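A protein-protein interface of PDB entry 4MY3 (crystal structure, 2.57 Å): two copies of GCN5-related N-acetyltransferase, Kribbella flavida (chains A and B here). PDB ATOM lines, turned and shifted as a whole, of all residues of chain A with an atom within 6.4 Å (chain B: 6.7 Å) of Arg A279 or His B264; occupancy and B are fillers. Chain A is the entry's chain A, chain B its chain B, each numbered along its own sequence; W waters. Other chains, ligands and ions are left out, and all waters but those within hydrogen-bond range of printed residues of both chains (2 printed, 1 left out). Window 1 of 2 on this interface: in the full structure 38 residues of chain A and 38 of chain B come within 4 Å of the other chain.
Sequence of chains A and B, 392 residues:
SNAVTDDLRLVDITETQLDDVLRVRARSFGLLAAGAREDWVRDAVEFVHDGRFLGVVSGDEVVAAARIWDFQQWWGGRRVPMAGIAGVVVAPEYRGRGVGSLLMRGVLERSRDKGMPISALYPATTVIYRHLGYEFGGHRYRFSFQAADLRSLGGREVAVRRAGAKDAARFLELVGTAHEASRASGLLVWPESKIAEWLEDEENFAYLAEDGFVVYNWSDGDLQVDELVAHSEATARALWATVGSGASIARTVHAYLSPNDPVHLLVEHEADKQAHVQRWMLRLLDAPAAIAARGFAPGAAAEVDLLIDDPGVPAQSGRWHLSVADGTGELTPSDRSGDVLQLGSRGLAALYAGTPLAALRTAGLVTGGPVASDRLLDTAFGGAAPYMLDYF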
ATOM      1  N   LEU A 121       9.785   1.504  25.591  1.00  0.00           N
ATOM      2  CA  LEU A 121      10.112   0.092  25.675  1.00  0.00           C
ATOM      3  C   LEU A 121      11.524  -0.110  25.143  1.00  0.00           C
ATOM      4  O   LEU A 121      12.005   0.715  24.347  1.00  0.00           O
ATOM      5  CB  LEU A 121       9.077  -0.765  24.907  1.00  0.00           C
ATOM      6  CG  LEU A 121       8.993  -1.002  23.374  1.00  0.00           C
ATOM      7  CD1 LEU A 121       7.528  -1.051  22.907  1.00  0.00           C
ATOM      8  CD2 LEU A 121       9.775  -0.027  22.497  1.00  0.00           C
ATOM      9  N   TYR A 122      12.179  -1.184  25.592  1.00  0.00           N
ATOM     10  CA  TYR A 122      13.436  -1.634  25.000  1.00  0.00           C
ATOM     11  C   TYR A 122      13.113  -2.658  23.926  1.00  0.00           C
ATOM     12  O   TYR A 122      12.495  -3.682  24.195  1.00  0.00           O
ATOM     13  CB  TYR A 122      14.350  -2.255  26.048  1.00  0.00           C
ATOM     14  CG  TYR A 122      15.076  -1.251  26.889  1.00  0.00           C
ATOM     15  CD1 TYR A 122      16.251  -0.658  26.445  1.00  0.00           C
ATOM     16  CD2 TYR A 122      14.585  -0.904  28.149  1.00  0.00           C
ATOM     17  CE1 TYR A 122      16.910   0.262  27.229  1.00  0.00           C
ATOM     18  CE2 TYR A 122      15.242   0.002  28.954  1.00  0.00           C
ATOM     19  CZ  TYR A 122      16.397   0.589  28.496  1.00  0.00           C
ATOM     20  OH  TYR A 122      17.026   1.501  29.325  1.00  0.00           O
ATOM     21  N   PRO A 123      13.506  -2.372  22.695  1.00  0.00           N
ATOM     22  CA  PRO A 123      12.985  -3.157  21.574  1.00  0.00           C
ATOM     23  C   PRO A 123      13.849  -4.376  21.245  1.00  0.00           C
ATOM     24  O   PRO A 123      15.049  -4.237  21.054  1.00  0.00           O
ATOM     25  CB  PRO A 123      13.020  -2.152  20.424  1.00  0.00           C
ATOM     26  CG  PRO A 123      14.154  -1.224  20.760  1.00  0.00           C
ATOM     27  CD  PRO A 123      14.305  -1.217  22.265  1.00  0.00           C
ATOM     28  N   ARG A 130       8.599   0.036  15.130  1.00  0.00           N
ATOM     29  CA  ARG A 130       8.583   1.206  14.287  1.00  0.00           C
ATOM     30  C   ARG A 130       7.250   1.282  13.534  1.00  0.00           C
ATOM     31  O   ARG A 130       6.600   2.326  13.523  1.00  0.00           O
ATOM     32  CB  ARG A 130       9.791   1.236  13.357  1.00  0.00           C
ATOM     33  CG  ARG A 130      11.071   1.637  14.062  1.00  0.00           C
ATOM     34  CD  ARG A 130      12.234   1.795  13.090  1.00  0.00           C
ATOM     35  NE  ARG A 130      13.324   2.573  13.684  1.00  0.00           N
ATOM     36  CZ  ARG A 130      14.618   2.258  13.607  1.00  0.00           C
ATOM     37  NH1 ARG A 130      15.017   1.170  12.950  1.00  0.00           N
ATOM     38  NH2 ARG A 130      15.518   3.039  14.186  1.00  0.00           N
ATOM     39  N   GLU A 135      10.033   5.082  18.275  1.00  0.00           N
ATOM     40  CA  GLU A 135      11.335   5.457  17.755  1.00  0.00           C
ATOM     41  C   GLU A 135      12.305   5.732  18.896  1.00  0.00           C
ATOM     42  O   GLU A 135      11.879   6.137  19.966  1.00  0.00           O
ATOM     43  CB  GLU A 135      11.224   6.676  16.827  1.00  0.00           C
ATOM     44  CG  GLU A 135      12.486   6.953  16.011  1.00  0.00           C
ATOM     45  CD  GLU A 135      13.002   5.696  15.318  1.00  0.00           C
ATOM     46  OE1 GLU A 135      13.885   5.016  15.893  1.00  0.00           O
ATOM     47  OE2 GLU A 135      12.513   5.380  14.206  1.00  0.00           O
ATOM     48  N   PHE A 136      13.598   5.502  18.671  1.00  0.00           N
ATOM     49  CA  PHE A 136      14.597   5.745  19.703  1.00  0.00           C
ATOM     50  C   PHE A 136      14.510   7.171  20.266  1.00  0.00           C
ATOM     51  O   PHE A 136      14.513   8.160  19.523  1.00  0.00           O
ATOM     52  CB  PHE A 136      16.017   5.461  19.193  1.00  0.00           C
ATOM     53  CG  PHE A 136      16.273   4.011  18.881  1.00  0.00           C
ATOM     54  CD1 PHE A 136      16.104   3.035  19.857  1.00  0.00           C
ATOM     55  CD2 PHE A 136      16.682   3.620  17.614  1.00  0.00           C
ATOM     56  CE1 PHE A 136      16.346   1.691  19.572  1.00  0.00           C
ATOM     57  CE2 PHE A 136      16.915   2.281  17.330  1.00  0.00           C
ATOM     58  CZ  PHE A 136      16.754   1.319  18.309  1.00  0.00           C
ATOM     59  N   GLY A 137      14.431   7.258  21.594  1.00  0.00           N
ATOM     60  CA  GLY A 137      14.290   8.528  22.266  1.00  0.00           C
ATOM     61  C   GLY A 137      15.384   8.791  23.274  1.00  0.00           C
ATOM     62  O   GLY A 137      15.581   9.936  23.667  1.00  0.00           O
ATOM     63  N   GLY A 138      16.111   7.758  23.689  1.00  0.00           N
ATOM     64  CA  GLY A 138      17.181   7.969  24.645  1.00  0.00           C
ATOM     65  C   GLY A 138      18.177   6.837  24.754  1.00  0.00           C
ATOM     66  O   GLY A 138      18.220   5.967  23.875  1.00  0.00           O
ATOM     67  N   HIS A 139      18.968   6.846  25.836  1.00  0.00           N
ATOM     68  CA  HIS A 139      20.041   5.873  26.039  1.00  0.00           C
ATOM     69  C   HIS A 139      20.111   5.385  27.481  1.00  0.00           C
ATOM     70  O   HIS A 139      19.603   6.038  28.392  1.00  0.00           O
ATOM     71  CB  HIS A 139      21.404   6.476  25.682  1.00  0.00           C
ATOM     72  CG  HIS A 139      21.534   6.928  24.260  1.00  0.00           C
ATOM     73  ND1 HIS A 139      21.277   8.225  23.860  1.00  0.00           N
ATOM     74  CD2 HIS A 139      21.922   6.266  23.146  1.00  0.00           C
ATOM     75  CE1 HIS A 139      21.484   8.335  22.563  1.00  0.00           C
ATOM     76  NE2 HIS A 139      21.878   7.159  22.104  1.00  0.00           N
ATOM     77  N   ARG A 140      20.730   4.221  27.679  1.00  0.00           N
ATOM     78  CA  ARG A 140      21.236   3.818  28.985  1.00  0.00           C
ATOM     79  C   ARG A 140      22.735   3.523  28.868  1.00  0.00           C
ATOM     80  O   ARG A 140      23.164   2.755  27.999  1.00  0.00           O
ATOM     81  CB  ARG A 140      20.505   2.590  29.534  1.00  0.00           C
ATOM     82  CG  ARG A 140      21.235   1.983  30.745  1.00  0.00           C
ATOM     83  CD  ARG A 140      20.372   1.062  31.617  1.00  0.00           C
ATOM     84  NE  ARG A 140      20.518  -0.328  31.199  1.00  0.00           N
ATOM     85  CZ  ARG A 140      20.702  -1.366  32.010  1.00  0.00           C
ATOM     86  NH1 ARG A 140      20.755  -1.213  33.328  1.00  0.00           N
ATOM     87  NH2 ARG A 140      20.823  -2.569  31.478  1.00  0.00           N
ATOM     88  N   VAL A 277      26.193   0.878  25.557  1.00  0.00           N
ATOM     89  CA  VAL A 277      25.261   1.925  25.176  1.00  0.00           C
ATOM     90  C   VAL A 277      23.995   1.311  24.589  1.00  0.00           C
ATOM     91  O   VAL A 277      23.980   0.882  23.425  1.00  0.00           O
ATOM     92  CB  VAL A 277      25.877   2.887  24.151  1.00  0.00           C
ATOM     93  CG1 VAL A 277      24.841   3.877  23.671  1.00  0.00           C
ATOM     94  CG2 VAL A 277      27.082   3.604  24.732  1.00  0.00           C
ATOM     95  N   GLN A 278      22.935   1.261  25.394  1.00  0.00           N
ATOM     96  CA  GLN A 278      21.660   0.743  24.915  1.00  0.00           C
ATOM     97  C   GLN A 278      20.704   1.879  24.607  1.00  0.00           C
ATOM     98  O   GLN A 278      20.862   2.979  25.103  1.00  0.00           O
ATOM     99  CB  GLN A 278      21.044  -0.170  25.948  1.00  0.00           C
ATOM    100  CG  GLN A 278      21.852  -1.386  26.218  1.00  0.00           C
ATOM    101  CD  GLN A 278      21.417  -2.039  27.491  1.00  0.00           C
ATOM    102  OE1 GLN A 278      21.724  -1.541  28.570  1.00  0.00           O
ATOM    103  NE2 GLN A 278      20.671  -3.143  27.386  1.00  0.00           N
ATOM    104  N   ARG A 279      19.704   1.598  23.790  1.00  0.00           N
ATOM    105  CA  ARG A 279      18.749   2.594  23.367  1.00  0.00           C
ATOM    106  C   ARG A 279      17.326   2.167  23.728  1.00  0.00           C
ATOM    107  O   ARG A 279      16.998   0.978  23.680  1.00  0.00           O
ATOM    108  CB  ARG A 279      18.866   2.766  21.864  1.00  0.00           C
ATOM    109  CG  ARG A 279      20.050   3.584  21.433  1.00  0.00           C
ATOM    110  CD  ARG A 279      20.338   3.342  19.965  1.00  0.00           C
ATOM    111  NE  ARG A 279      21.572   2.587  19.865  1.00  0.00           N
ATOM    112  CZ  ARG A 279      22.737   3.157  19.660  1.00  0.00           C
ATOM    113  NH1 ARG A 279      22.792   4.467  19.510  1.00  0.00           N
ATOM    114  NH2 ARG A 279      23.824   2.429  19.604  1.00  0.00           N
ATOM    115  N   TRP A 280      16.481   3.132  24.090  1.00  0.00           N
ATOM    116  CA  TRP A 280      15.080   2.828  24.344  1.00  0.00           C
ATOM    117  C   TRP A 280      14.225   3.703  23.449  1.00  0.00           C
ATOM    118  O   TRP A 280      14.639   4.800  23.072  1.00  0.00           O
ATOM    119  CB  TRP A 280      14.717   3.000  25.836  1.00  0.00           C
ATOM    120  CG  TRP A 280      15.241   4.285  26.462  1.00  0.00           C
ATOM    121  CD1 TRP A 280      16.421   4.455  27.125  1.00  0.00           C
ATOM    122  CD2 TRP A 280      14.590   5.564  26.475  1.00  0.00           C
ATOM    123  NE1 TRP A 280      16.550   5.764  27.542  1.00  0.00           N
ATOM    124  CE2 TRP A 280      15.439   6.461  27.151  1.00  0.00           C
ATOM    125  CE3 TRP A 280      13.377   6.040  25.963  1.00  0.00           C
ATOM    126  CZ2 TRP A 280      15.117   7.801  27.321  1.00  0.00           C
ATOM    127  CZ3 TRP A 280      13.057   7.369  26.143  1.00  0.00           C
ATOM    128  CH2 TRP A 280      13.922   8.234  26.809  1.00  0.00           C
ATOM    129  N   MET A 281      13.043   3.211  23.091  1.00  0.00           N
ATOM    130  CA  MET A 281      12.151   3.939  22.202  1.00  0.00           C
ATOM    131  C   MET A 281      11.032   4.654  22.943  1.00  0.00           C
ATOM    132  O   MET A 281      10.749   4.356  24.112  1.00  0.00           O
ATOM    133  CB  MET A 281      11.541   3.001  21.176  1.00  0.00           C
ATOM    134  CG  MET A 281      12.542   2.460  20.158  1.00  0.00           C
ATOM    135  SD  MET A 281      11.723   1.270  18.797  1.00  0.00           S
ATOM    136  CE  MET A 281      13.130   1.420  17.438  1.00  0.00           C
ATOM    137  N   PHE B 143      30.734   3.239  16.992  1.00  0.00           N
ATOM    138  CA  PHE B 143      29.621   2.292  17.042  1.00  0.00           C
ATOM    139  C   PHE B 143      29.777   1.258  15.953  1.00  0.00           C
ATOM    140  O   PHE B 143      30.403   1.540  14.928  1.00  0.00           O
ATOM    141  CB  PHE B 143      28.280   3.005  16.882  1.00  0.00           C
ATOM    142  CG  PHE B 143      27.952   3.924  18.018  1.00  0.00           C
ATOM    143  CD1 PHE B 143      27.582   3.410  19.250  1.00  0.00           C
ATOM    144  CD2 PHE B 143      28.008   5.303  17.855  1.00  0.00           C
ATOM    145  CE1 PHE B 143      27.276   4.257  20.309  1.00  0.00           C
ATOM    146  CE2 PHE B 143      27.709   6.147  18.903  1.00  0.00           C
ATOM    147  CZ  PHE B 143      27.345   5.626  20.132  1.00  0.00           C
ATOM    148  N   PHE B 145      28.068  -1.733  13.347  1.00  0.00           N
ATOM    149  CA  PHE B 145      26.864  -2.113  12.658  1.00  0.00           C
ATOM    150  C   PHE B 145      27.019  -3.434  11.947  1.00  0.00           C
ATOM    151  O   PHE B 145      28.135  -3.861  11.646  1.00  0.00           O
ATOM    152  CB  PHE B 145      26.469  -0.999  11.701  1.00  0.00           C
ATOM    153  CG  PHE B 145      26.169   0.274  12.393  1.00  0.00           C
ATOM    154  CD1 PHE B 145      24.965   0.444  13.056  1.00  0.00           C
ATOM    155  CD2 PHE B 145      27.107   1.289  12.441  1.00  0.00           C
ATOM    156  CE1 PHE B 145      24.689   1.626  13.734  1.00  0.00           C
ATOM    157  CE2 PHE B 145      26.836   2.480  13.124  1.00  0.00           C
ATOM    158  CZ  PHE B 145      25.627   2.645  13.772  1.00  0.00           C
ATOM    159  N   LEU B 257      31.063   8.431  14.685  1.00  0.00           N
ATOM    160  CA  LEU B 257      29.986   9.391  14.497  1.00  0.00           C
ATOM    161  C   LEU B 257      29.358   9.850  15.820  1.00  0.00           C
ATOM    162  O   LEU B 257      29.642   9.294  16.881  1.00  0.00           O
ATOM    163  CB  LEU B 257      28.921   8.827  13.553  1.00  0.00           C
ATOM    164  CG  LEU B 257      28.687   7.320  13.492  1.00  0.00           C
ATOM    165  CD1 LEU B 257      27.705   6.901  14.549  1.00  0.00           C
ATOM    166  CD2 LEU B 257      28.200   6.907  12.120  1.00  0.00           C
ATOM    167  N   SER B 258      28.530  10.889  15.744  1.00  0.00           N
ATOM    168  CA  SER B 258      27.722  11.340  16.871  1.00  0.00           C
ATOM    169  C   SER B 258      26.738  10.249  17.315  1.00  0.00           C
ATOM    170  O   SER B 258      26.425   9.327  16.553  1.00  0.00           O
ATOM    171  CB  SER B 258      26.960  12.604  16.462  1.00  0.00           C
ATOM    172  OG  SER B 258      25.689  12.681  17.087  1.00  0.00           O
ATOM    173  N   PRO B 259      26.250  10.330  18.560  1.00  0.00           N
ATOM    174  CA  PRO B 259      25.183   9.389  18.921  1.00  0.00           C
ATOM    175  C   PRO B 259      23.837   9.933  18.442  1.00  0.00           C
ATOM    176  O   PRO B 259      22.810   9.259  18.566  1.00  0.00           O
ATOM    177  CB  PRO B 259      25.232   9.355  20.457  1.00  0.00           C
ATOM    178  CG  PRO B 259      26.457  10.134  20.855  1.00  0.00           C
ATOM    179  CD  PRO B 259      26.727  11.091  19.724  1.00  0.00           C
ATOM    180  N   ASN B 260      23.844  11.144  17.893  1.00  0.00           N
ATOM    181  CA  ASN B 260      22.645  11.679  17.271  1.00  0.00           C
ATOM    182  C   ASN B 260      22.619  11.500  15.749  1.00  0.00           C
ATOM    183  O   ASN B 260      21.776  12.073  15.061  1.00  0.00           O
ATOM    184  CB  ASN B 260      22.467  13.142  17.649  1.00  0.00           C
ATOM    185  CG  ASN B 260      22.043  13.314  19.092  1.00  0.00           C
ATOM    186  OD1 ASN B 260      21.224  12.538  19.612  1.00  0.00           O
ATOM    187  ND2 ASN B 260      22.604  14.322  19.756  1.00  0.00           N
ATOM    188  N   ASP B 261      23.544  10.703  15.226  1.00  0.00           N
ATOM    189  CA  ASP B 261      23.604  10.460  13.800  1.00  0.00           C
ATOM    190  C   ASP B 261      22.333   9.809  13.321  1.00  0.00           C
ATOM    191  O   ASP B 261      21.718   9.042  14.050  1.00  0.00           O
ATOM    192  CB  ASP B 261      24.772   9.543  13.472  1.00  0.00           C
ATOM    193  CG  ASP B 261      25.117   9.566  12.014  1.00  0.00           C
ATOM    194  OD1 ASP B 261      26.090  10.248  11.642  1.00  0.00           O
ATOM    195  OD2 ASP B 261      24.383   8.939  11.234  1.00  0.00           O
ATOM    196  N   PRO B 262      21.926  10.116  12.091  1.00  0.00           N
ATOM    197  CA  PRO B 262      20.710   9.525  11.544  1.00  0.00           C
ATOM    198  C   PRO B 262      20.744   8.010  11.357  1.00  0.00           C
ATOM    199  O   PRO B 262      19.638   7.458  11.288  1.00  0.00           O
ATOM    200  CB  PRO B 262      20.584  10.206  10.185  1.00  0.00           C
ATOM    201  CG  PRO B 262      21.259  11.512  10.360  1.00  0.00           C
ATOM    202  CD  PRO B 262      22.383  11.269  11.293  1.00  0.00           C
ATOM    203  N   VAL B 263      21.909   7.356  11.251  1.00  0.00           N
ATOM    204  CA  VAL B 263      21.892   5.902  11.000  1.00  0.00           C
ATOM    205  C   VAL B 263      21.039   5.213  12.030  1.00  0.00           C
ATOM    206  O   VAL B 263      20.230   4.360  11.697  1.00  0.00           O
ATOM    207  CB  VAL B 263      23.250   5.160  11.107  1.00  0.00           C
ATOM    208  CG1 VAL B 263      23.573   4.434   9.806  1.00  0.00           C
ATOM    209  CG2 VAL B 263      24.351   6.036  11.580  1.00  0.00           C
ATOM    210  N   HIS B 264      21.230   5.600  13.285  1.00  0.00           N
ATOM    211  CA  HIS B 264      20.483   5.019  14.379  1.00  0.00           C
ATOM    212  C   HIS B 264      18.984   4.981  14.116  1.00  0.00           C
ATOM    213  O   HIS B 264      18.303   4.098  14.614  1.00  0.00           O
ATOM    214  CB  HIS B 264      20.804   5.755  15.668  1.00  0.00           C
ATOM    215  CG  HIS B 264      22.251   5.705  16.029  1.00  0.00           C
ATOM    216  ND1 HIS B 264      22.968   4.528  16.064  1.00  0.00           N
ATOM    217  CD2 HIS B 264      23.120   6.685  16.363  1.00  0.00           C
ATOM    218  CE1 HIS B 264      24.219   4.781  16.408  1.00  0.00           C
ATOM    219  NE2 HIS B 264      24.337   6.082  16.596  1.00  0.00           N
ATOM    220  N   LEU B 265      18.481   5.915  13.310  1.00  0.00           N
ATOM    221  CA  LEU B 265      17.055   5.987  13.023  1.00  0.00           C
ATOM    222  C   LEU B 265      16.676   5.177  11.790  1.00  0.00           C
ATOM    223  O   LEU B 265      15.499   4.895  11.576  1.00  0.00           O
ATOM    224  CB  LEU B 265      16.613   7.443  12.853  1.00  0.00           C
ATOM    225  CG  LEU B 265      16.849   8.356  14.061  1.00  0.00           C
ATOM    226  CD1 LEU B 265      16.625   9.802  13.698  1.00  0.00           C
ATOM    227  CD2 LEU B 265      15.951   7.960  15.230  1.00  0.00           C
ATOM    228  N   LEU B 266      17.669   4.791  10.990  1.00  0.00           N
ATOM    229  CA  LEU B 266      17.417   4.114   9.727  1.00  0.00           C
ATOM    230  C   LEU B 266      17.656   2.612   9.746  1.00  0.00           C
ATOM    231  O   LEU B 266      16.956   1.877   9.054  1.00  0.00           O
ATOM    232  CB  LEU B 266      18.286   4.708   8.632  1.00  0.00           C
ATOM    233  CG  LEU B 266      18.055   6.151   8.205  1.00  0.00           C
ATOM    234  CD1 LEU B 266      19.350   6.713   7.611  1.00  0.00           C
ATOM    235  CD2 LEU B 266      16.889   6.265   7.224  1.00  0.00           C
ATOM    236  N   VAL B 267      18.655   2.151  10.496  1.00  0.00           N
ATOM    237  CA  VAL B 267      19.084   0.755  10.422  1.00  0.00           C
ATOM    238  C   VAL B 267      18.062  -0.183  11.070  1.00  0.00           C
ATOM    239  O   VAL B 267      17.343   0.212  11.972  1.00  0.00           O
ATOM    240  CB  VAL B 267      20.490   0.561  11.084  1.00  0.00           C
ATOM    241  CG1 VAL B 267      21.128  -0.706  10.621  1.00  0.00           C
ATOM    242  CG2 VAL B 267      21.403   1.660  10.705  1.00  0.00           C
ATOM    243  N   HIS B 269      18.778  -3.217  12.684  1.00  0.00           N
ATOM    244  CA  HIS B 269      19.284  -3.739  13.944  1.00  0.00           C
ATOM    245  C   HIS B 269      20.042  -2.634  14.668  1.00  0.00           C
ATOM    246  O   HIS B 269      20.824  -1.903  14.075  1.00  0.00           O
ATOM    247  CB  HIS B 269      20.154  -5.004  13.738  1.00  0.00           C
ATOM    248  CG  HIS B 269      19.411  -6.153  13.125  1.00  0.00           C
ATOM    249  ND1 HIS B 269      19.413  -6.410  11.766  1.00  0.00           N
ATOM    250  CD2 HIS B 269      18.610  -7.096  13.681  1.00  0.00           C
ATOM    251  CE1 HIS B 269      18.647  -7.458  11.512  1.00  0.00           C
ATOM    252  NE2 HIS B 269      18.153  -7.897  12.658  1.00  0.00           N
ATOM    253  N   GLU B 270      19.797  -2.504  15.958  1.00  0.00           N
ATOM    254  CA  GLU B 270      20.468  -1.490  16.749  1.00  0.00           C
ATOM    255  C   GLU B 270      21.982  -1.703  16.698  1.00  0.00           C
ATOM    256  O   GLU B 270      22.436  -2.832  16.550  1.00  0.00           O
ATOM    257  CB  GLU B 270      19.965  -1.604  18.176  1.00  0.00           C
ATOM    258  CG  GLU B 270      20.409  -0.517  19.083  1.00  0.00           C
ATOM    259  CD  GLU B 270      19.834  -0.695  20.469  1.00  0.00           C
ATOM    260  OE1 GLU B 270      20.333   0.000  21.379  1.00  0.00           O
ATOM    261  OE2 GLU B 270      18.889  -1.518  20.644  1.00  0.00           O
ATOM    262  N   ALA B 271      22.763  -0.631  16.791  1.00  0.00           N
ATOM    263  CA  ALA B 271      24.219  -0.758  16.909  1.00  0.00           C
ATOM    264  C   ALA B 271      24.523  -1.646  18.103  1.00  0.00           C
ATOM    265  O   ALA B 271      23.750  -1.651  19.063  1.00  0.00           O
ATOM    266  CB  ALA B 271      24.873   0.610  17.097  1.00  0.00           C
ATOM    267  N   ASP B 272      25.624  -2.394  18.062  1.00  0.00           N
ATOM    268  CA  ASP B 272      25.932  -3.297  19.167  1.00  0.00           C
ATOM    269  C   ASP B 272      26.081  -2.510  20.460  1.00  0.00           C
ATOM    270  O   ASP B 272      26.640  -1.416  20.477  1.00  0.00           O
ATOM    271  CB  ASP B 272      27.198  -4.127  18.919  1.00  0.00           C
ATOM    272  CG  ASP B 272      27.075  -5.056  17.710  1.00  0.00           C
ATOM    273  OD1 ASP B 272      25.954  -5.219  17.161  1.00  0.00           O
ATOM    274  OD2 ASP B 272      28.116  -5.637  17.313  1.00  0.00           O
ATOM    275  N   LYS B 273      25.559  -3.083  21.534  1.00  0.00           N
ATOM    276  CA  LYS B 273      25.658  -2.508  22.856  1.00  0.00           C
ATOM    277  C   LYS B 273      27.084  -2.064  23.212  1.00  0.00           C
ATOM    278  O   LYS B 273      27.271  -1.032  23.865  1.00  0.00           O
ATOM    279  CB  LYS B 273      25.152  -3.529  23.867  1.00  0.00           C
ATOM    280  CG  LYS B 273      25.278  -3.075  25.280  1.00  0.00           C
ATOM    281  CD  LYS B 273      24.484  -3.956  26.192  1.00  0.00           C
ATOM    282  CE  LYS B 273      25.046  -5.354  26.237  1.00  0.00           C
ATOM    283  NZ  LYS B 273      24.694  -5.973  27.534  1.00  0.00           N
ATOM    284  N   ALA B 275      30.488  -0.378  22.773  1.00  0.00           N
ATOM    285  CA  ALA B 275      30.936   0.773  21.985  1.00  0.00           C
ATOM    286  C   ALA B 275      32.184   1.413  22.569  1.00  0.00           C
ATOM    287  O   ALA B 275      32.603   1.064  23.672  1.00  0.00           O
ATOM    288  CB  ALA B 275      29.814   1.808  21.864  1.00  0.00           C
HETATM  289  O   HOH W   1      17.197  -3.218  19.481  1.00  0.00           O
HETATM  290  O   HOH W   2      25.432   1.212  20.993  1.00  0.00           O
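Hydrophobic or aromatic side chains of chain B within 4 Å of the printed part of chain A: Phe B143, His B264, Leu B265 and Ala B271. Of the 15 printed residues of chain A, 6 touch a printed residue of chain B. Among the printed residues, 12 pairs touch across the chains.
Water W2 lies within hydrogen-bond range of NH2 of Arg A279, O of Val A277 and O of Asp B272. Water W1 lies within hydrogen-bond range of the side-chain carboxylate of Glu B270 (2.7 Å) and the backbone carbonyl oxygen of Pro A123 (2.9 Å).
Arg A279 touches just these residues of chain B: Phe B143, His B264, Glu B270 and Ala B271. Of chain A, only Arg A130, Phe A136 and Arg A279 come within 4 Å of His B264. Printed residues of chain A within 4 Å of Ala B271: Arg A279. Of the printed residues of chain A, Leu B265 touches Arg A130 (3.2 Å) and Glu A135 (3.7 Å). Trp A280 touches none of the printed residues of chain B.
The guanidinium group of Arg A130 is in hydrogen-bond range of the backbone carbonyl oxygen of His B264 (3.0 Å). NH2 of Arg A130 is in hydrogen-bond range of O of Leu B265 (3.2 Å). O of Val B267 is in hydrogen-bond range of NH1 of Arg A130 (2.7 Å). O of Lys B273 is in hydrogen-bond range of N of Val A277, at 2.8 Å. ND1 of His B264 lies close to NH1 of Arg A279, at 3.5 Å. NE of Arg A279 lies within salt-bridge range of OE1 of Glu B270, 3.2 Å away.
OE1 of Glu A135 touches CD2 of Leu B265 (3.7 Å). O of His B264 touches CD2 of Phe A136 (3.4 Å). C of Gln A278 touches OE1 of Glu B270, at 3.8 Å. Lys B273 touches Gln A278 (CD to CG, 3.7 Å). Phe B143 touches Arg A279 (CD1 to NH2, 3.9 Å). Arg A279 touches Ala B271 (NH2 to CB, 3.3 Å).
The side-chain carboxylate (OE2) of Glu A135 lies within salt-bridge range of the guanidinium group (NE) of Arg A130 (3.0 Å). The backbone NH of Arg A140 lies within hydrogen-bond range of the backbone carbonyl oxygen of Gln A278 (2.9 Å).
No position is printed for both chains. Of the 12 pairs that touch across the chains among the printed residues, none has its exchanged pair printed and touching as well.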
